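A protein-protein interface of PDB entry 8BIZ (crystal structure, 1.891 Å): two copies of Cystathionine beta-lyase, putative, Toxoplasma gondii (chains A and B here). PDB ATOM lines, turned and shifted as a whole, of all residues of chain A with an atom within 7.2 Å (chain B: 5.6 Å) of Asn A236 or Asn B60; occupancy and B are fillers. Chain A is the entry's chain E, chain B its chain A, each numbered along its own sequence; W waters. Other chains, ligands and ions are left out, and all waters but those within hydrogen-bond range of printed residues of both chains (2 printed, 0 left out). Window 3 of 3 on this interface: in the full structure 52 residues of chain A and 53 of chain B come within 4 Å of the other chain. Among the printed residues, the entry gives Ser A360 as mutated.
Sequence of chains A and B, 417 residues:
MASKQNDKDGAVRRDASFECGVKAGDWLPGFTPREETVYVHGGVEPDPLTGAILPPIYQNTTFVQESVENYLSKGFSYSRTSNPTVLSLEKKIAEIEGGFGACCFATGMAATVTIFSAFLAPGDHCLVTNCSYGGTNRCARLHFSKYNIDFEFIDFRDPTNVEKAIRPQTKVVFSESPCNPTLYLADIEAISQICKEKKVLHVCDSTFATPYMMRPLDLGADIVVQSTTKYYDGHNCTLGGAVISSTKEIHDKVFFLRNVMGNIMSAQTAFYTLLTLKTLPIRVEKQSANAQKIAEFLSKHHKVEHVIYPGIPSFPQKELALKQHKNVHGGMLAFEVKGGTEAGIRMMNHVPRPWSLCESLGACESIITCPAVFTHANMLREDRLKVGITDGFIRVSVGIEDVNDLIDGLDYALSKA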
ATOM      1  N   THR A 229      24.956  -5.558  25.281  1.00  0.00           N
ATOM      2  CA  THR A 229      24.538  -6.285  24.081  1.00  0.00           C
ATOM      3  C   THR A 229      23.438  -5.554  23.320  1.00  0.00           C
ATOM      4  O   THR A 229      23.401  -5.572  22.081  1.00  0.00           O
ATOM      5  CB  THR A 229      24.024  -7.671  24.489  1.00  0.00           C
ATOM      6  OG1 THR A 229      24.980  -8.306  25.350  1.00  0.00           O
ATOM      7  CG2 THR A 229      23.727  -8.530  23.272  1.00  0.00           C
ATOM      8  N   LYS A 230      22.528  -4.913  24.048  1.00  0.00           N
ATOM      9  CA  LYS A 230      21.266  -4.474  23.470  1.00  0.00           C
ATOM     10  C   LYS A 230      21.420  -3.124  22.782  1.00  0.00           C
ATOM     11  O   LYS A 230      21.615  -3.074  21.565  1.00  0.00           O
ATOM     12  CB  LYS A 230      20.195  -4.434  24.560  1.00  0.00           C
ATOM     13  CG  LYS A 230      20.065  -5.748  25.330  1.00  0.00           C
ATOM     14  CD  LYS A 230      19.913  -6.929  24.396  1.00  0.00           C
ATOM     15  CE  LYS A 230      20.059  -8.271  25.121  1.00  0.00           C
ATOM     16  NZ  LYS A 230      19.135  -8.391  26.284  1.00  0.00           N
ATOM     17  N   ASP A 233      25.549  -1.499  22.194  1.00  0.00           N
ATOM     18  CA  ASP A 233      25.972  -2.064  20.916  1.00  0.00           C
ATOM     19  C   ASP A 233      25.004  -1.607  19.826  1.00  0.00           C
ATOM     20  O   ASP A 233      25.369  -0.835  18.929  1.00  0.00           O
ATOM     21  CB  ASP A 233      26.020  -3.598  21.013  1.00  0.00           C
ATOM     22  CG  ASP A 233      26.557  -4.261  19.745  1.00  0.00           C
ATOM     23  OD1 ASP A 233      27.645  -4.872  19.788  1.00  0.00           O
ATOM     24  OD2 ASP A 233      25.918  -4.135  18.684  1.00  0.00           O
ATOM     25  N   GLY A 234      23.767  -2.084  19.887  1.00  0.00           N
ATOM     26  CA  GLY A 234      22.742  -1.607  18.973  1.00  0.00           C
ATOM     27  C   GLY A 234      22.913  -2.082  17.548  1.00  0.00           C
ATOM     28  O   GLY A 234      22.144  -1.678  16.675  1.00  0.00           O
ATOM     29  N   HIS A 235      23.892  -2.945  17.290  1.00  0.00           N
ATOM     30  CA  HIS A 235      24.158  -3.391  15.930  1.00  0.00           C
ATOM     31  C   HIS A 235      24.127  -4.909  15.811  1.00  0.00           C
ATOM     32  O   HIS A 235      24.540  -5.437  14.775  1.00  0.00           O
ATOM     33  CB  HIS A 235      25.512  -2.859  15.464  1.00  0.00           C
ATOM     34  CG  HIS A 235      25.532  -1.382  15.211  1.00  0.00           C
ATOM     35  ND1 HIS A 235      25.550  -0.457  16.231  1.00  0.00           N
ATOM     36  CD2 HIS A 235      25.586  -0.670  14.057  1.00  0.00           C
ATOM     37  CE1 HIS A 235      25.594   0.761  15.720  1.00  0.00           C
ATOM     38  NE2 HIS A 235      25.631   0.657  14.402  1.00  0.00           N
ATOM     39  N   ASN A 236      23.656  -5.622  16.837  1.00  0.00           N
ATOM     40  CA  ASN A 236      23.624  -7.089  16.849  1.00  0.00           C
ATOM     41  C   ASN A 236      25.017  -7.692  16.734  1.00  0.00           C
ATOM     42  O   ASN A 236      25.165  -8.837  16.316  1.00  0.00           O
ATOM     43  CB  ASN A 236      22.709  -7.639  15.745  1.00  0.00           C
ATOM     44  CG  ASN A 236      21.267  -7.662  16.158  1.00  0.00           C
ATOM     45  OD1 ASN A 236      20.954  -8.119  17.260  1.00  0.00           O
ATOM     46  ND2 ASN A 236      20.375  -7.148  15.310  1.00  0.00           N
ATOM     47  N   CYS A 237      26.042  -6.939  17.140  1.00  0.00           N
ATOM     48  CA  CYS A 237      27.437  -7.290  16.887  1.00  0.00           C
ATOM     49  C   CYS A 237      28.092  -8.029  18.052  1.00  0.00           C
ATOM     50  O   CYS A 237      28.659  -9.107  17.856  1.00  0.00           O
ATOM     51  CB  CYS A 237      28.217  -6.009  16.546  1.00  0.00           C
ATOM     52  SG  CYS A 237      29.916  -6.402  16.065  1.00  0.00           S
ATOM     53  N   THR A 238      28.035  -7.480  19.266  1.00  0.00           N
ATOM     54  CA  THR A 238      28.790  -8.028  20.384  1.00  0.00           C
ATOM     55  C   THR A 238      27.861  -8.403  21.534  1.00  0.00           C
ATOM     56  O   THR A 238      26.740  -7.905  21.633  1.00  0.00           O
ATOM     57  CB  THR A 238      29.838  -7.026  20.893  1.00  0.00           C
ATOM     58  OG1 THR A 238      29.176  -5.970  21.595  1.00  0.00           O
ATOM     59  CG2 THR A 238      30.603  -6.415  19.748  1.00  0.00           C
ATOM     60  N   LEU A 239      28.339  -9.291  22.394  1.00  0.00           N
ATOM     61  CA  LEU A 239      27.772  -9.471  23.722  1.00  0.00           C
ATOM     62  C   LEU A 239      28.562  -8.635  24.727  1.00  0.00           C
ATOM     63  O   LEU A 239      29.773  -8.458  24.603  1.00  0.00           O
ATOM     64  CB  LEU A 239      27.835 -10.940  24.162  1.00  0.00           C
ATOM     65  CG  LEU A 239      27.166 -12.017  23.312  1.00  0.00           C
ATOM     66  CD1 LEU A 239      27.616 -13.376  23.803  1.00  0.00           C
ATOM     67  CD2 LEU A 239      25.661 -11.883  23.415  1.00  0.00           C
ATOM     68  N   SER A 356      12.880  -9.160  11.660  1.00  0.00           N
ATOM     69  CA  SER A 356      13.621 -10.389  11.935  1.00  0.00           C
ATOM     70  C   SER A 356      12.921 -11.108  13.085  1.00  0.00           C
ATOM     71  O   SER A 356      12.604 -10.492  14.108  1.00  0.00           O
ATOM     72  CB  SER A 356      15.083 -10.095  12.282  1.00  0.00           C
ATOM     73  OG  SER A 356      15.769  -9.502  11.186  1.00  0.00           O
ATOM     74  N   CYS A 358      13.397 -13.383  15.984  1.00  0.00           N
ATOM     75  CA  CYS A 358      14.530 -13.864  16.772  1.00  0.00           C
ATOM     76  C   CYS A 358      14.514 -13.225  18.155  1.00  0.00           C
ATOM     77  O   CYS A 358      13.666 -12.385  18.469  1.00  0.00           O
ATOM     78  CB  CYS A 358      15.844 -13.594  16.044  1.00  0.00           C
ATOM     79  SG  CYS A 358      16.068 -11.808  15.744  1.00  0.00           S
ATOM     80  N   GLU A 359      15.458 -13.654  18.993  1.00  0.00           N
ATOM     81  CA  GLU A 359      15.643 -13.090  20.319  1.00  0.00           C
ATOM     82  C   GLU A 359      16.488 -11.822  20.225  1.00  0.00           C
ATOM     83  O   GLU A 359      16.907 -11.412  19.140  1.00  0.00           O
ATOM     84  CB  GLU A 359      16.268 -14.135  21.247  1.00  0.00           C
ATOM     85  CG  GLU A 359      15.282 -15.272  21.569  1.00  0.00           C
ATOM     86  CD  GLU A 359      15.929 -16.617  21.913  1.00  0.00           C
ATOM     87  OE1 GLU A 359      15.237 -17.665  21.766  1.00  0.00           O
ATOM     88  OE2 GLU A 359      17.108 -16.654  22.344  1.00  0.00           O
ATOM     89  N   SER A 360      16.710 -11.202  21.387  1.00  0.00           N
ATOM     90  CA  SER A 360      17.455  -9.962  21.606  1.00  0.00           C
ATOM     91  C   SER A 360      16.636  -8.732  21.218  1.00  0.00           C
ATOM     92  O   SER A 360      15.469  -8.846  20.829  1.00  0.00           O
ATOM     93  CB  SER A 360      18.794  -9.950  20.870  1.00  0.00           C
ATOM     94  OG  SER A 360      19.689  -9.066  21.530  1.00  0.00           O
ATOM     95  N   LEU A 361      17.246  -7.558  21.325  1.00  0.00           N
ATOM     96  CA  LEU A 361      16.536  -6.291  21.193  1.00  0.00           C
ATOM     97  C   LEU A 361      17.559  -5.165  21.151  1.00  0.00           C
ATOM     98  O   LEU A 361      18.743  -5.364  21.440  1.00  0.00           O
ATOM     99  CB  LEU A 361      15.560  -6.090  22.361  1.00  0.00           C
ATOM    100  CG  LEU A 361      16.239  -6.105  23.744  1.00  0.00           C
ATOM    101  CD1 LEU A 361      16.358  -4.732  24.377  1.00  0.00           C
ATOM    102  CD2 LEU A 361      15.541  -7.093  24.674  1.00  0.00           C
ATOM    103  N   GLY A 362      17.078  -3.977  20.785  1.00  0.00           N
ATOM    104  CA  GLY A 362      17.859  -2.763  20.893  1.00  0.00           C
ATOM    105  C   GLY A 362      18.612  -2.373  19.643  1.00  0.00           C
ATOM    106  O   GLY A 362      19.290  -1.348  19.643  1.00  0.00           O
ATOM    107  N   ALA A 363      18.503  -3.149  18.577  1.00  0.00           N
ATOM    108  CA  ALA A 363      19.388  -3.050  17.428  1.00  0.00           C
ATOM    109  C   ALA A 363      18.801  -2.193  16.304  1.00  0.00           C
ATOM    110  O   ALA A 363      17.604  -1.894  16.272  1.00  0.00           O
ATOM    111  CB  ALA A 363      19.698  -4.449  16.898  1.00  0.00           C
ATOM    112  N   CYS A 364      19.687  -1.800  15.375  1.00  0.00           N
ATOM    113  CA  CYS A 364      19.286  -1.151  14.126  1.00  0.00           C
ATOM    114  C   CYS A 364      18.265  -1.973  13.359  1.00  0.00           C
ATOM    115  O   CYS A 364      17.416  -1.412  12.657  1.00  0.00           O
ATOM    116  CB  CYS A 364      20.509  -0.938  13.235  1.00  0.00           C
ATOM    117  SG  CYS A 364      21.654   0.283  13.935  1.00  0.00           S
ATOM    118  N   GLU A 365      18.370  -3.299  13.448  1.00  0.00           N
ATOM    119  CA  GLU A 365      17.452  -4.217  12.788  1.00  0.00           C
ATOM    120  C   GLU A 365      16.250  -4.485  13.693  1.00  0.00           C
ATOM    121  O   GLU A 365      16.419  -4.921  14.835  1.00  0.00           O
ATOM    122  CB  GLU A 365      18.189  -5.521  12.455  1.00  0.00           C
ATOM    123  CG  GLU A 365      19.372  -5.317  11.505  1.00  0.00           C
ATOM    124  CD  GLU A 365      20.718  -5.060  12.178  1.00  0.00           C
ATOM    125  OE1 GLU A 365      21.714  -5.058  11.438  1.00  0.00           O
ATOM    126  OE2 GLU A 365      20.816  -4.922  13.420  1.00  0.00           O
ATOM    127  N   SER A 366      15.045  -4.209  13.189  1.00  0.00           N
ATOM    128  CA  SER A 366      13.835  -4.413  13.979  1.00  0.00           C
ATOM    129  C   SER A 366      13.637  -5.903  14.245  1.00  0.00           C
ATOM    130  O   SER A 366      13.830  -6.732  13.354  1.00  0.00           O
ATOM    131  CB  SER A 366      12.613  -3.827  13.268  1.00  0.00           C
ATOM    132  OG  SER A 366      12.659  -2.410  13.232  1.00  0.00           O
ATOM    133  N   ILE A 367      13.256  -6.232  15.477  1.00  0.00           N
ATOM    134  CA  ILE A 367      13.155  -7.605  15.953  1.00  0.00           C
ATOM    135  C   ILE A 367      11.783  -7.806  16.577  1.00  0.00           C
ATOM    136  O   ILE A 367      11.271  -6.927  17.274  1.00  0.00           O
ATOM    137  CB  ILE A 367      14.273  -7.930  16.968  1.00  0.00           C
ATOM    138  CG1 ILE A 367      15.639  -7.915  16.283  1.00  0.00           C
ATOM    139  CG2 ILE A 367      14.018  -9.267  17.656  1.00  0.00           C
ATOM    140  CD1 ILE A 367      16.803  -7.947  17.252  1.00  0.00           C
ATOM    141  N   TYR B  58      31.535 -15.814  13.312  1.00  0.00           N
ATOM    142  CA  TYR B  58      30.150 -15.407  13.553  1.00  0.00           C
ATOM    143  C   TYR B  58      30.119 -14.316  14.623  1.00  0.00           C
ATOM    144  O   TYR B  58      29.809 -14.541  15.796  1.00  0.00           O
ATOM    145  CB  TYR B  58      29.292 -16.600  13.935  1.00  0.00           C
ATOM    146  CG  TYR B  58      28.992 -17.450  12.745  1.00  0.00           C
ATOM    147  CD1 TYR B  58      27.883 -17.192  11.950  1.00  0.00           C
ATOM    148  CD2 TYR B  58      29.845 -18.484  12.378  1.00  0.00           C
ATOM    149  CE1 TYR B  58      27.616 -17.956  10.845  1.00  0.00           C
ATOM    150  CE2 TYR B  58      29.583 -19.250  11.276  1.00  0.00           C
ATOM    151  CZ  TYR B  58      28.470 -18.984  10.511  1.00  0.00           C
ATOM    152  OH  TYR B  58      28.204 -19.756   9.407  1.00  0.00           O
ATOM    153  N   GLN B  59      30.474 -13.107  14.182  1.00  0.00           N
ATOM    154  CA  GLN B  59      30.461 -11.915  15.027  1.00  0.00           C
ATOM    155  C   GLN B  59      29.046 -11.333  15.015  1.00  0.00           C
ATOM    156  O   GLN B  59      28.754 -10.318  14.378  1.00  0.00           O
ATOM    157  CB  GLN B  59      31.489 -10.898  14.541  1.00  0.00           C
ATOM    158  CG  GLN B  59      31.645  -9.683  15.431  1.00  0.00           C
ATOM    159  CD  GLN B  59      32.319  -9.996  16.747  1.00  0.00           C
ATOM    160  OE1 GLN B  59      33.402 -10.566  16.775  1.00  0.00           O
ATOM    161  NE2 GLN B  59      31.662  -9.651  17.854  1.00  0.00           N
ATOM    162  N   ASN B  60      28.147 -12.014  15.724  1.00  0.00           N
ATOM    163  CA  ASN B  60      26.751 -11.608  15.766  1.00  0.00           C
ATOM    164  C   ASN B  60      26.102 -12.176  17.019  1.00  0.00           C
ATOM    165  O   ASN B  60      26.463 -13.253  17.494  1.00  0.00           O
ATOM    166  CB  ASN B  60      25.947 -12.064  14.542  1.00  0.00           C
ATOM    167  CG  ASN B  60      25.780 -13.553  14.496  1.00  0.00           C
ATOM    168  OD1 ASN B  60      26.743 -14.270  14.193  1.00  0.00           O
ATOM    169  ND2 ASN B  60      24.597 -14.051  14.891  1.00  0.00           N
ATOM    170  N   THR B  61      25.099 -11.458  17.519  1.00  0.00           N
ATOM    171  CA  THR B  61      24.493 -11.819  18.792  1.00  0.00           C
ATOM    172  C   THR B  61      23.323 -12.781  18.638  1.00  0.00           C
ATOM    173  O   THR B  61      23.154 -13.673  19.464  1.00  0.00           O
ATOM    174  CB  THR B  61      24.023 -10.562  19.520  1.00  0.00           C
ATOM    175  OG1 THR B  61      23.087  -9.874  18.689  1.00  0.00           O
ATOM    176  CG2 THR B  61      25.178  -9.660  19.763  1.00  0.00           C
ATOM    177  N   THR B  62      22.489 -12.603  17.621  1.00  0.00           N
ATOM    178  CA  THR B  62      21.233 -13.333  17.579  1.00  0.00           C
ATOM    179  C   THR B  62      21.035 -13.984  16.217  1.00  0.00           C
ATOM    180  O   THR B  62      21.653 -13.603  15.217  1.00  0.00           O
ATOM    181  CB  THR B  62      20.055 -12.411  17.939  1.00  0.00           C
ATOM    182  OG1 THR B  62      18.869 -13.193  18.123  1.00  0.00           O
ATOM    183  CG2 THR B  62      19.822 -11.354  16.873  1.00  0.00           C
ATOM    184  N   PHE B  63      20.175 -14.998  16.193  1.00  0.00           N
ATOM    185  CA  PHE B  63      20.004 -15.839  15.017  1.00  0.00           C
ATOM    186  C   PHE B  63      18.524 -15.913  14.667  1.00  0.00           C
ATOM    187  O   PHE B  63      17.686 -16.162  15.538  1.00  0.00           O
ATOM    188  CB  PHE B  63      20.583 -17.236  15.258  1.00  0.00           C
ATOM    189  CG  PHE B  63      22.058 -17.234  15.573  1.00  0.00           C
ATOM    190  CD1 PHE B  63      22.517 -16.868  16.833  1.00  0.00           C
ATOM    191  CD2 PHE B  63      22.983 -17.601  14.613  1.00  0.00           C
ATOM    192  CE1 PHE B  63      23.873 -16.858  17.125  1.00  0.00           C
ATOM    193  CE2 PHE B  63      24.340 -17.590  14.891  1.00  0.00           C
ATOM    194  CZ  PHE B  63      24.784 -17.217  16.148  1.00  0.00           C
ATOM    195  N   SER B  79      24.042 -15.818  21.158  1.00  0.00           N
ATOM    196  CA  SER B  79      25.463 -16.152  21.249  1.00  0.00           C
ATOM    197  C   SER B  79      25.942 -16.301  22.697  1.00  0.00           C
ATOM    198  O   SER B  79      27.022 -16.863  22.927  1.00  0.00           O
ATOM    199  CB  SER B  79      26.277 -15.095  20.504  1.00  0.00           C
ATOM    200  OG  SER B  79      26.369 -15.424  19.118  1.00  0.00           O
ATOM    201  N   ASN B  83      27.515 -20.298  20.110  1.00  0.00           N
ATOM    202  CA  ASN B  83      27.901 -19.577  18.909  1.00  0.00           C
ATOM    203  C   ASN B  83      28.615 -20.540  17.966  1.00  0.00           C
ATOM    204  O   ASN B  83      29.378 -21.392  18.430  1.00  0.00           O
ATOM    205  CB  ASN B  83      28.799 -18.397  19.292  1.00  0.00           C
ATOM    206  CG  ASN B  83      29.366 -17.680  18.090  1.00  0.00           C
ATOM    207  OD1 ASN B  83      30.310 -18.165  17.467  1.00  0.00           O
ATOM    208  ND2 ASN B  83      28.770 -16.538  17.732  1.00  0.00           N
ATOM    209  N   PRO B  84      28.389 -20.444  16.649  1.00  0.00           N
ATOM    210  CA  PRO B  84      28.965 -21.463  15.738  1.00  0.00           C
ATOM    211  C   PRO B  84      30.492 -21.525  15.741  1.00  0.00           C
ATOM    212  O   PRO B  84      31.069 -22.617  15.651  1.00  0.00           O
ATOM    213  CB  PRO B  84      28.428 -21.049  14.358  1.00  0.00           C
ATOM    214  CG  PRO B  84      27.226 -20.191  14.634  1.00  0.00           C
ATOM    215  CD  PRO B  84      27.525 -19.482  15.935  1.00  0.00           C
HETATM  216  O   HOH W   1      21.473  -8.009  19.858  1.00  0.00           O
HETATM  217  O   HOH W   2      16.920 -16.131  18.168  1.00  0.00           O
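Of the printed residues of chain B, Thr A229 touches Thr B61. Asp A233 touches none of the printed residues of chain B. Of chain B, only Asn B60 (3.2 Å), Thr B61 (2.9 Å) and Thr B62 (3.4 Å) come within 4 Å of Asn A236. Of the printed residues of chain B, Glu A359 touches Thr B62 (2.8 Å). Of chain A, only Asn A236 and Cys A237 come within 4 Å of Asn B60. Of the printed residues of chain A, Phe B63 touches Cys A358 (3.2 Å). The nearest residue of chain B that does not touch Asn A236 is Gln B59 (4.3 Å).
Of the 9 printed residues of chain B, 6 touch a printed residue of chain A. Hydrophobic or aromatic side chains of chain A that line the printed part of chain B: Leu A239. Among the printed residues, 13 pairs touch across the chains.
No position is printed for both chains. Of the 13 pairs that touch across the chains among the printed residues, none has its exchanged pair printed and touching as well.
Among the printed residues, merely in contact across the chains: Thr A229 with Thr B61 (3.96 Å), Asn A236 with Asn B60 (3.2 Å), Asn A236 with Thr B62 (3.4 Å), Cys A237 with Asn B60 (3.6 Å), Cys A237 with Thr B61 (3.8 Å), Thr A238 with Gln B59 (3.9 Å), Thr A238 with Thr B61 (3.0 Å), Leu A239 with Ser B79 (3.5 Å), Cys A358 with Thr B62 (3.7 Å) and Cys A358 with Phe B63 (3.2 Å).
Water W1 lies within hydrogen-bond range of OD1 of Asn A236, OG of Ser A360 and OG1 of Thr B61. Water W2 lies within hydrogen-bond range of O of Phe B63 and N of Glu A359.
The side-chain carboxylate of Asp A233 lies within hydrogen-bond range of the backbone NH of Asn A236 (3.3 Å). OD2 of Asp A233 is in hydrogen-bond range of N of Cys A237 (3.2 Å). The side-chain carboxylate (OD1) of Asp A233 lies within hydrogen-bond range of the side-chain hydroxyl (OG1) of Thr A238 (2.6 Å). ND2 of Asn A236 lies within hydrogen-bond range of OE2 of Glu A365 (3.0 Å). The backbone carbonyl oxygen (O) of Asn B60 is in hydrogen-bond range of the side-chain hydroxyl (OG) of Ser B79 (2.7 Å). The backbone carbonyl oxygen of Thr B61 sits at hydrogen-bond distance from the backbone NH of Ser B79, 2.9 Å away.
The backbone carbonyl oxygen (O) of Asn A236 lies within hydrogen-bond range of the backbone NH (N) of Thr B61, at 2.9 Å. The backbone carbonyl oxygen (O) of Cys A237 lies within hydrogen-bond range of the side-chain amide nitrogen (NE2) of Gln B59 (3.1 Å). The backbone carbonyl oxygen of Glu A359 is in hydrogen-bond range of the side-chain hydroxyl of Thr B62, 2.8 Å away.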
